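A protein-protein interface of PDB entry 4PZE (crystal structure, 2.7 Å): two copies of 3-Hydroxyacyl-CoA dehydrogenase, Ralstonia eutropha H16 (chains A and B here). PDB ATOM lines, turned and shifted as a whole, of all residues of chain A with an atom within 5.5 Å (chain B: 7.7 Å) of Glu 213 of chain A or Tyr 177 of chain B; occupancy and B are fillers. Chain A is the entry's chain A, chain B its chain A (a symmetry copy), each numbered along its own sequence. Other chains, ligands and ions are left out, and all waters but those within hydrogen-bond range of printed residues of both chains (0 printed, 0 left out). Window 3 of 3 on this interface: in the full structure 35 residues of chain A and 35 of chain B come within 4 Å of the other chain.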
ATOM      1  N   ALA A 209      11.216 -27.048  -8.578  1.00  0.00           N
ATOM      2  CA  ALA A 209       9.825 -26.757  -8.195  1.00  0.00           C
ATOM      3  C   ALA A 209       9.735 -26.358  -6.708  1.00  0.00           C
ATOM      4  O   ALA A 209      10.631 -26.633  -5.936  1.00  0.00           O
ATOM      5  CB  ALA A 209       8.953 -27.982  -8.459  1.00  0.00           C
ATOM      6  N   SER A 210       8.652 -25.723  -6.294  1.00  0.00           N
ATOM      7  CA  SER A 210       8.503 -25.347  -4.869  1.00  0.00           C
ATOM      8  C   SER A 210       8.167 -26.578  -4.003  1.00  0.00           C
ATOM      9  O   SER A 210       7.632 -27.571  -4.516  1.00  0.00           O
ATOM     10  CB  SER A 210       7.448 -24.241  -4.684  1.00  0.00           C
ATOM     11  OG  SER A 210       6.271 -24.515  -5.438  1.00  0.00           O
ATOM     12  N   PRO A 211       8.484 -26.519  -2.690  1.00  0.00           N
ATOM     13  CA  PRO A 211       8.129 -27.645  -1.819  1.00  0.00           C
ATOM     14  C   PRO A 211       6.619 -27.953  -1.827  1.00  0.00           C
ATOM     15  O   PRO A 211       6.226 -29.106  -1.981  1.00  0.00           O
ATOM     16  CB  PRO A 211       8.585 -27.207  -0.419  1.00  0.00           C
ATOM     17  CG  PRO A 211       9.331 -25.936  -0.582  1.00  0.00           C
ATOM     18  CD  PRO A 211       9.106 -25.396  -1.964  1.00  0.00           C
ATOM     19  N   GLU A 212       5.780 -26.938  -1.683  1.00  0.00           N
ATOM     20  CA  GLU A 212       4.330 -27.185  -1.604  1.00  0.00           C
ATOM     21  C   GLU A 212       3.814 -27.846  -2.874  1.00  0.00           C
ATOM     22  O   GLU A 212       2.932 -28.684  -2.795  1.00  0.00           O
ATOM     23  CB  GLU A 212       3.526 -25.907  -1.331  1.00  0.00           C
ATOM     24  CG  GLU A 212       3.876 -25.168  -0.041  1.00  0.00           C
ATOM     25  CD  GLU A 212       5.046 -24.190  -0.163  1.00  0.00           C
ATOM     26  OE1 GLU A 212       5.464 -23.883  -1.304  1.00  0.00           O
ATOM     27  OE2 GLU A 212       5.554 -23.713   0.887  1.00  0.00           O
ATOM     28  N   GLU A 213       4.365 -27.470  -4.034  1.00  0.00           N
ATOM     29  CA  GLU A 213       3.970 -28.062  -5.357  1.00  0.00           C
ATOM     30  C   GLU A 213       4.564 -29.453  -5.647  1.00  0.00           C
ATOM     31  O   GLU A 213       3.981 -30.224  -6.344  1.00  0.00           O
ATOM     32  CB  GLU A 213       4.348 -27.122  -6.515  1.00  0.00           C
ATOM     33  CG  GLU A 213       3.553 -25.821  -6.563  1.00  0.00           C
ATOM     34  CD  GLU A 213       3.860 -24.987  -7.792  1.00  0.00           C
ATOM     35  OE1 GLU A 213       5.003 -25.099  -8.321  1.00  0.00           O
ATOM     36  OE2 GLU A 213       2.952 -24.221  -8.218  1.00  0.00           O
ATOM     37  N   ILE A 214       5.741 -29.736  -5.119  1.00  0.00           N
ATOM     38  CA  ILE A 214       6.321 -31.047  -5.166  1.00  0.00           C
ATOM     39  C   ILE A 214       5.391 -31.965  -4.409  1.00  0.00           C
ATOM     40  O   ILE A 214       5.082 -33.080  -4.852  1.00  0.00           O
ATOM     41  CB  ILE A 214       7.719 -31.040  -4.495  1.00  0.00           C
ATOM     42  CG1 ILE A 214       8.778 -30.490  -5.460  1.00  0.00           C
ATOM     43  CG2 ILE A 214       8.138 -32.436  -4.037  1.00  0.00           C
ATOM     44  CD1 ILE A 214      10.154 -30.348  -4.835  1.00  0.00           C
ATOM     45  N   ASP A 215       4.971 -31.486  -3.241  1.00  0.00           N
ATOM     46  CA  ASP A 215       4.189 -32.285  -2.309  1.00  0.00           C
ATOM     47  C   ASP A 215       2.818 -32.499  -2.911  1.00  0.00           C
ATOM     48  O   ASP A 215       2.224 -33.530  -2.717  1.00  0.00           O
ATOM     49  CB  ASP A 215       4.080 -31.593  -0.950  1.00  0.00           C
ATOM     50  CG  ASP A 215       5.157 -32.043   0.072  1.00  0.00           C
ATOM     51  OD1 ASP A 215       6.004 -32.932  -0.216  1.00  0.00           O
ATOM     52  OD2 ASP A 215       5.120 -31.517   1.220  1.00  0.00           O
ATOM     53  N   GLU A 216       2.319 -31.544  -3.678  1.00  0.00           N
ATOM     54  CA  GLU A 216       0.956 -31.671  -4.175  1.00  0.00           C
ATOM     55  C   GLU A 216       0.947 -32.588  -5.379  1.00  0.00           C
ATOM     56  O   GLU A 216       0.078 -33.482  -5.508  1.00  0.00           O
ATOM     57  CB  GLU A 216       0.307 -30.300  -4.458  1.00  0.00           C
ATOM     58  CG  GLU A 216      -0.582 -29.837  -3.305  1.00  0.00           C
ATOM     59  CD  GLU A 216      -1.545 -28.737  -3.700  1.00  0.00           C
ATOM     60  OE1 GLU A 216      -2.684 -28.737  -3.178  1.00  0.00           O
ATOM     61  OE2 GLU A 216      -1.170 -27.878  -4.535  1.00  0.00           O
ATOM     62  N   GLY A 217       1.938 -32.376  -6.241  1.00  0.00           N
ATOM     63  CA  GLY A 217       2.243 -33.316  -7.299  1.00  0.00           C
ATOM     64  C   GLY A 217       2.123 -34.778  -6.891  1.00  0.00           C
ATOM     65  O   GLY A 217       1.488 -35.559  -7.589  1.00  0.00           O
ATOM     66  N   MET A 218       2.728 -35.149  -5.768  1.00  0.00           N
ATOM     67  CA  MET A 218       2.716 -36.548  -5.331  1.00  0.00           C
ATOM     68  C   MET A 218       1.378 -36.947  -4.694  1.00  0.00           C
ATOM     69  O   MET A 218       0.954 -38.112  -4.849  1.00  0.00           O
ATOM     70  CB  MET A 218       3.884 -36.854  -4.349  1.00  0.00           C
ATOM     71  CG  MET A 218       5.293 -36.596  -4.890  1.00  0.00           C
ATOM     72  SD  MET A 218       5.747 -37.404  -6.447  1.00  0.00           S
ATOM     73  CE  MET A 218       5.717 -39.084  -5.840  1.00  0.00           C
ATOM     74  N   LEU A 220      -1.813 -35.520  -5.285  1.00  0.00           N
ATOM     75  CA  LEU A 220      -2.819 -35.620  -6.325  1.00  0.00           C
ATOM     76  C   LEU A 220      -2.445 -36.601  -7.424  1.00  0.00           C
ATOM     77  O   LEU A 220      -3.318 -37.297  -7.970  1.00  0.00           O
ATOM     78  CB  LEU A 220      -3.022 -34.256  -6.967  1.00  0.00           C
ATOM     79  CG  LEU A 220      -3.617 -33.207  -6.041  1.00  0.00           C
ATOM     80  CD1 LEU A 220      -3.182 -31.837  -6.489  1.00  0.00           C
ATOM     81  CD2 LEU A 220      -5.121 -33.316  -6.009  1.00  0.00           C
ATOM     82  N   PHE B 142      -2.643 -35.872 -16.379  1.00  0.00           N
ATOM     83  CA  PHE B 142      -2.620 -37.236 -15.853  1.00  0.00           C
ATOM     84  C   PHE B 142      -3.823 -38.066 -16.296  1.00  0.00           C
ATOM     85  O   PHE B 142      -4.884 -37.530 -16.595  1.00  0.00           O
ATOM     86  CB  PHE B 142      -2.368 -37.231 -14.357  1.00  0.00           C
ATOM     87  CG  PHE B 142      -0.943 -36.860 -14.018  1.00  0.00           C
ATOM     88  CD1 PHE B 142      -0.494 -35.553 -14.181  1.00  0.00           C
ATOM     89  CD2 PHE B 142      -0.039 -37.818 -13.590  1.00  0.00           C
ATOM     90  CE1 PHE B 142       0.811 -35.218 -13.895  1.00  0.00           C
ATOM     91  CE2 PHE B 142       1.262 -37.481 -13.286  1.00  0.00           C
ATOM     92  CZ  PHE B 142       1.689 -36.186 -13.437  1.00  0.00           C
ATOM     93  N   MET B 148      -8.704 -36.347 -12.853  1.00  0.00           N
ATOM     94  CA  MET B 148      -7.425 -35.990 -12.189  1.00  0.00           C
ATOM     95  C   MET B 148      -7.254 -34.473 -12.126  1.00  0.00           C
ATOM     96  O   MET B 148      -7.309 -33.785 -13.152  1.00  0.00           O
ATOM     97  CB  MET B 148      -6.204 -36.587 -12.914  1.00  0.00           C
ATOM     98  CG  MET B 148      -6.188 -38.101 -12.998  1.00  0.00           C
ATOM     99  SD  MET B 148      -6.065 -38.902 -11.389  1.00  0.00           S
ATOM    100  CE  MET B 148      -4.521 -39.807 -11.588  1.00  0.00           C
ATOM    101  N   ALA B 149      -7.020 -33.953 -10.927  1.00  0.00           N
ATOM    102  CA  ALA B 149      -7.040 -32.527 -10.730  1.00  0.00           C
ATOM    103  C   ALA B 149      -5.651 -31.904 -10.768  1.00  0.00           C
ATOM    104  O   ALA B 149      -5.370 -30.982  -9.992  1.00  0.00           O
ATOM    105  CB  ALA B 149      -7.735 -32.212  -9.413  1.00  0.00           C
ATOM    106  N   LEU B 150      -4.781 -32.369 -11.665  1.00  0.00           N
ATOM    107  CA  LEU B 150      -3.439 -31.777 -11.765  1.00  0.00           C
ATOM    108  C   LEU B 150      -2.708 -31.909 -13.082  1.00  0.00           C
ATOM    109  O   LEU B 150      -2.859 -32.891 -13.816  1.00  0.00           O
ATOM    110  CB  LEU B 150      -2.539 -32.283 -10.641  1.00  0.00           C
ATOM    111  CG  LEU B 150      -1.936 -33.693 -10.606  1.00  0.00           C
ATOM    112  CD1 LEU B 150      -2.651 -34.705 -11.493  1.00  0.00           C
ATOM    113  CD2 LEU B 150      -0.446 -33.634 -10.911  1.00  0.00           C
ATOM    114  N   VAL B 151      -1.919 -30.874 -13.355  1.00  0.00           N
ATOM    115  CA  VAL B 151      -1.067 -30.768 -14.534  1.00  0.00           C
ATOM    116  C   VAL B 151       0.345 -30.351 -14.113  1.00  0.00           C
ATOM    117  O   VAL B 151       0.517 -29.467 -13.259  1.00  0.00           O
ATOM    118  CB  VAL B 151      -1.548 -29.645 -15.451  1.00  0.00           C
ATOM    119  CG1 VAL B 151      -0.868 -29.746 -16.816  1.00  0.00           C
ATOM    120  CG2 VAL B 151      -3.054 -29.670 -15.577  1.00  0.00           C
ATOM    121  N   GLU B 152       1.357 -30.966 -14.716  1.00  0.00           N
ATOM    122  CA  GLU B 152       2.721 -30.481 -14.580  1.00  0.00           C
ATOM    123  C   GLU B 152       2.864 -29.470 -15.706  1.00  0.00           C
ATOM    124  O   GLU B 152       2.528 -29.772 -16.838  1.00  0.00           O
ATOM    125  CB  GLU B 152       3.754 -31.621 -14.666  1.00  0.00           C
ATOM    126  CG  GLU B 152       3.959 -32.408 -13.360  1.00  0.00           C
ATOM    127  CD  GLU B 152       5.000 -33.552 -13.456  1.00  0.00           C
ATOM    128  OE1 GLU B 152       5.115 -34.219 -14.510  1.00  0.00           O
ATOM    129  OE2 GLU B 152       5.719 -33.805 -12.457  1.00  0.00           O
ATOM    130  N   LEU B 153       3.283 -28.252 -15.369  1.00  0.00           N
ATOM    131  CA  LEU B 153       3.527 -27.180 -16.331  1.00  0.00           C
ATOM    132  C   LEU B 153       5.022 -27.048 -16.384  1.00  0.00           C
ATOM    133  O   LEU B 153       5.649 -26.715 -15.382  1.00  0.00           O
ATOM    134  CB  LEU B 153       2.969 -25.849 -15.829  1.00  0.00           C
ATOM    135  CG  LEU B 153       1.468 -25.650 -15.653  1.00  0.00           C
ATOM    136  CD1 LEU B 153       1.203 -24.276 -15.035  1.00  0.00           C
ATOM    137  CD2 LEU B 153       0.762 -25.803 -16.997  1.00  0.00           C
ATOM    138  N   HIS B 164       4.053 -18.401 -19.309  1.00  0.00           N
ATOM    139  CA  HIS B 164       3.807 -19.227 -18.128  1.00  0.00           C
ATOM    140  C   HIS B 164       2.500 -18.833 -17.457  1.00  0.00           C
ATOM    141  O   HIS B 164       1.602 -19.666 -17.339  1.00  0.00           O
ATOM    142  CB  HIS B 164       4.995 -19.175 -17.152  1.00  0.00           C
ATOM    143  CG  HIS B 164       4.668 -19.633 -15.766  1.00  0.00           C
ATOM    144  ND1 HIS B 164       4.405 -20.948 -15.457  1.00  0.00           N
ATOM    145  CD2 HIS B 164       4.565 -18.942 -14.604  1.00  0.00           C
ATOM    146  CE1 HIS B 164       4.140 -21.046 -14.166  1.00  0.00           C
ATOM    147  NE2 HIS B 164       4.233 -19.844 -13.625  1.00  0.00           N
ATOM    148  N   GLU B 168      -0.630 -21.042 -16.872  1.00  0.00           N
ATOM    149  CA  GLU B 168      -0.934 -21.225 -15.432  1.00  0.00           C
ATOM    150  C   GLU B 168      -2.421 -20.984 -15.157  1.00  0.00           C
ATOM    151  O   GLU B 168      -3.084 -21.806 -14.520  1.00  0.00           O
ATOM    152  CB  GLU B 168      -0.092 -20.299 -14.530  1.00  0.00           C
ATOM    153  CG  GLU B 168      -0.194 -20.620 -13.035  1.00  0.00           C
ATOM    154  CD  GLU B 168       0.802 -19.839 -12.175  1.00  0.00           C
ATOM    155  OE1 GLU B 168       1.048 -18.635 -12.433  1.00  0.00           O
ATOM    156  OE2 GLU B 168       1.340 -20.427 -11.213  1.00  0.00           O
ATOM    157  N   SER B 171      -4.864 -23.570 -16.909  1.00  0.00           N
ATOM    158  CA  SER B 171      -4.939 -24.794 -16.120  1.00  0.00           C
ATOM    159  C   SER B 171      -5.886 -24.615 -14.947  1.00  0.00           C
ATOM    160  O   SER B 171      -6.763 -25.441 -14.734  1.00  0.00           O
ATOM    161  CB  SER B 171      -3.555 -25.184 -15.608  1.00  0.00           C
ATOM    162  OG  SER B 171      -2.572 -24.587 -16.419  1.00  0.00           O
ATOM    163  N   LYS B 172      -5.690 -23.532 -14.190  1.00  0.00           N
ATOM    164  CA  LYS B 172      -6.558 -23.200 -13.049  1.00  0.00           C
ATOM    165  C   LYS B 172      -8.035 -23.120 -13.439  1.00  0.00           C
ATOM    166  O   LYS B 172      -8.886 -23.525 -12.657  1.00  0.00           O
ATOM    167  CB  LYS B 172      -6.113 -21.894 -12.367  1.00  0.00           C
ATOM    168  CG  LYS B 172      -5.034 -22.064 -11.296  1.00  0.00           C
ATOM    169  CD  LYS B 172      -4.581 -20.720 -10.722  1.00  0.00           C
ATOM    170  CE  LYS B 172      -3.846 -20.849  -9.395  1.00  0.00           C
ATOM    171  NZ  LYS B 172      -2.408 -21.183  -9.577  1.00  0.00           N
ATOM    172  N   LEU B 174      -9.471 -24.843 -16.087  1.00  0.00           N
ATOM    173  CA  LEU B 174      -9.779 -26.272 -16.324  1.00  0.00           C
ATOM    174  C   LEU B 174     -10.079 -27.096 -15.069  1.00  0.00           C
ATOM    175  O   LEU B 174     -10.597 -28.201 -15.183  1.00  0.00           O
ATOM    176  CB  LEU B 174      -8.659 -26.949 -17.124  1.00  0.00           C
ATOM    177  CG  LEU B 174      -8.882 -27.005 -18.641  1.00  0.00           C
ATOM    178  CD1 LEU B 174      -9.056 -25.615 -19.236  1.00  0.00           C
ATOM    179  CD2 LEU B 174      -7.750 -27.749 -19.341  1.00  0.00           C
ATOM    180  N   GLY B 175      -9.736 -26.563 -13.892  1.00  0.00           N
ATOM    181  CA  GLY B 175     -10.149 -27.124 -12.605  1.00  0.00           C
ATOM    182  C   GLY B 175      -9.112 -28.011 -11.941  1.00  0.00           C
ATOM    183  O   GLY B 175      -9.453 -28.788 -11.034  1.00  0.00           O
ATOM    184  N   LYS B 176      -7.853 -27.890 -12.381  1.00  0.00           N
ATOM    185  CA  LYS B 176      -6.743 -28.713 -11.878  1.00  0.00           C
ATOM    186  C   LYS B 176      -5.795 -27.831 -11.075  1.00  0.00           C
ATOM    187  O   LYS B 176      -5.660 -26.656 -11.385  1.00  0.00           O
ATOM    188  CB  LYS B 176      -5.915 -29.338 -13.025  1.00  0.00           C
ATOM    189  CG  LYS B 176      -6.584 -29.518 -14.382  1.00  0.00           C
ATOM    190  CD  LYS B 176      -7.617 -30.627 -14.372  1.00  0.00           C
ATOM    191  CE  LYS B 176      -7.366 -31.580 -15.521  1.00  0.00           C
ATOM    192  NZ  LYS B 176      -8.440 -32.602 -15.625  1.00  0.00           N
ATOM    193  N   TYR B 177      -5.127 -28.383 -10.065  1.00  0.00           N
ATOM    194  CA  TYR B 177      -3.978 -27.690  -9.501  1.00  0.00           C
ATOM    195  C   TYR B 177      -2.796 -27.928 -10.444  1.00  0.00           C
ATOM    196  O   TYR B 177      -2.488 -29.062 -10.755  1.00  0.00           O
ATOM    197  CB  TYR B 177      -3.636 -28.123  -8.053  1.00  0.00           C
ATOM    198  CG  TYR B 177      -2.598 -27.193  -7.447  1.00  0.00           C
ATOM    199  CD1 TYR B 177      -1.247 -27.366  -7.723  1.00  0.00           C
ATOM    200  CD2 TYR B 177      -2.972 -26.090  -6.677  1.00  0.00           C
ATOM    201  CE1 TYR B 177      -0.291 -26.499  -7.227  1.00  0.00           C
ATOM    202  CE2 TYR B 177      -2.018 -25.210  -6.175  1.00  0.00           C
ATOM    203  CZ  TYR B 177      -0.672 -25.420  -6.451  1.00  0.00           C
ATOM    204  OH  TYR B 177       0.305 -24.566  -5.963  1.00  0.00           O
ATOM    205  N   PRO B 178      -2.141 -26.856 -10.910  1.00  0.00           N
ATOM    206  CA  PRO B 178      -0.917 -26.942 -11.702  1.00  0.00           C
ATOM    207  C   PRO B 178       0.378 -26.872 -10.903  1.00  0.00           C
ATOM    208  O   PRO B 178       0.593 -25.909 -10.177  1.00  0.00           O
ATOM    209  CB  PRO B 178      -0.992 -25.691 -12.550  1.00  0.00           C
ATOM    210  CG  PRO B 178      -1.654 -24.698 -11.663  1.00  0.00           C
ATOM    211  CD  PRO B 178      -2.650 -25.477 -10.858  1.00  0.00           C
ATOM    212  N   ILE B 179       1.229 -27.881 -11.060  1.00  0.00           N
ATOM    213  CA  ILE B 179       2.612 -27.849 -10.581  1.00  0.00           C
ATOM    214  C   ILE B 179       3.426 -27.105 -11.626  1.00  0.00           C
ATOM    215  O   ILE B 179       3.104 -27.214 -12.805  1.00  0.00           O
ATOM    216  CB  ILE B 179       3.187 -29.286 -10.480  1.00  0.00           C
ATOM    217  CG1 ILE B 179       2.336 -30.172  -9.554  1.00  0.00           C
ATOM    218  CG2 ILE B 179       4.646 -29.270 -10.046  1.00  0.00           C
ATOM    219  CD1 ILE B 179       1.752 -29.448  -8.363  1.00  0.00           C
ATOM    220  N   THR B 180       4.457 -26.349 -11.219  1.00  0.00           N
ATOM    221  CA  THR B 180       5.421 -25.721 -12.173  1.00  0.00           C
ATOM    222  C   THR B 180       6.835 -26.308 -11.998  1.00  0.00           C
ATOM    223  O   THR B 180       7.317 -26.497 -10.875  1.00  0.00           O
ATOM    224  CB  THR B 180       5.416 -24.172 -12.102  1.00  0.00           C
ATOM    225  OG1 THR B 180       4.500 -23.658 -13.078  1.00  0.00           O
ATOM    226  CG2 THR B 180       6.803 -23.552 -12.389  1.00  0.00           C
ATOM    227  N   VAL B 181       7.485 -26.623 -13.116  1.00  0.00           N
ATOM    228  CA  VAL B 181       8.695 -27.443 -13.072  1.00  0.00           C
ATOM    229  C   VAL B 181       9.586 -26.932 -14.144  1.00  0.00           C
ATOM    230  O   VAL B 181       9.111 -26.750 -15.246  1.00  0.00           O
ATOM    231  CB  VAL B 181       8.419 -28.940 -13.372  1.00  0.00           C
ATOM    232  CG1 VAL B 181       9.635 -29.783 -13.068  1.00  0.00           C
ATOM    233  CG2 VAL B 181       7.253 -29.465 -12.544  1.00  0.00           C
ATOM    234  N   VAL B 188       8.583 -33.757 -12.125  1.00  0.00           N
ATOM    235  CA  VAL B 188       8.497 -33.942 -10.694  1.00  0.00           C
ATOM    236  C   VAL B 188       7.920 -35.305 -10.343  1.00  0.00           C
ATOM    237  O   VAL B 188       8.525 -36.083  -9.601  1.00  0.00           O
ATOM    238  CB  VAL B 188       7.686 -32.787 -10.071  1.00  0.00           C
ATOM    239  CG1 VAL B 188       7.229 -33.105  -8.646  1.00  0.00           C
ATOM    240  CG2 VAL B 188       8.522 -31.514 -10.098  1.00  0.00           C
ATOM    241  N   VAL B 189       6.748 -35.618 -10.868  1.00  0.00           N
ATOM    242  CA  VAL B 189       6.056 -36.793 -10.390  1.00  0.00           C
ATOM    243  C   VAL B 189       6.876 -38.009 -10.729  1.00  0.00           C
ATOM    244  O   VAL B 189       7.277 -38.776  -9.834  1.00  0.00           O
ATOM    245  CB  VAL B 189       4.645 -36.905 -10.947  1.00  0.00           C
ATOM    246  CG1 VAL B 189       4.031 -38.232 -10.545  1.00  0.00           C
ATOM    247  CG2 VAL B 189       3.790 -35.755 -10.410  1.00  0.00           C
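The backbone NH (N) of Thr 180 of chain B sits at hydrogen-bond distance from the side-chain carboxylate (OE1) of Glu 213 of chain A, 3.2 Å away.
OH of Tyr 177 of chain B is in hydrogen-bond range of OE2 of Glu 213 of chain A (3.5 Å).
The backbone NH (N) of Val 188 of chain B sits at hydrogen-bond distance from the side-chain carboxylate (OE2) of Glu 152 of chain B, at 2.9 Å.
N of Leu 153 of chain B lies within hydrogen-bond range of O of Ile 179 of chain B (2.8 Å).
O of Tyr 177 of chain B sits at hydrogen-bond distance from N of Val 151 of chain B, 3.2 Å away.
O of Val 151 of chain B lies within hydrogen-bond range of N of Ile 179 of chain B, 2.8 Å away.
The side-chain carboxylate (OE2) of Glu 152 of chain B sits at hydrogen-bond distance from the backbone NH (N) of Val 189 of chain B, 2.6 Å away.
N of Tyr 177 of chain B sits at hydrogen-bond distance from O of Ala 149 of chain B, at 2.6 Å.
Among the printed residues, pairs that only touch across the chains: Glu 213 of chain A with Ile 179 of chain B (3.1 Å), Glu 216 of chain A with Tyr 177 of chain B (3.1 Å), Ala 209 of chain A with Thr 180 of chain B (3.3 Å), Glu 213 of chain A with Pro 178 of chain B (3.5 Å), Gly 217 of chain A with Ile 179 of chain B (3.6 Å), Gly 217 of chain A with Val 189 of chain B (3.6 Å), Leu 220 of chain A with Leu 150 of chain B (3.8 Å), Ala 209 of chain A with Val 188 of chain B (3.9 Å) and Met 218 of chain A with Val 189 of chain B (3.96 Å).
Of the printed residues of chain B, Glu 216 of chain A touches Tyr 177.
Of the printed residues of chain B, Met 218 of chain A touches Val 189.
Phe 142 of chain B touches none of the printed residues of chain A.
Tyr 177 of chain B touches two residues of chain A.
Of the printed residues of chain A, Ile 179 of chain B touches Glu 213 and Gly 217.
Of the printed residues of chain A, Thr 180 of chain B touches Ala 209 and Glu 213.
The nearest residue of chain A that does not touch Tyr 177 of chain B is Leu 220 of chain A (4.1 Å).
Printed residues of chain B that touch a printed residue of chain A: Leu 150, Tyr 177, Pro 178, Ile 179, Thr 180, Val 188 and Val 189.
No position is printed for both chains.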
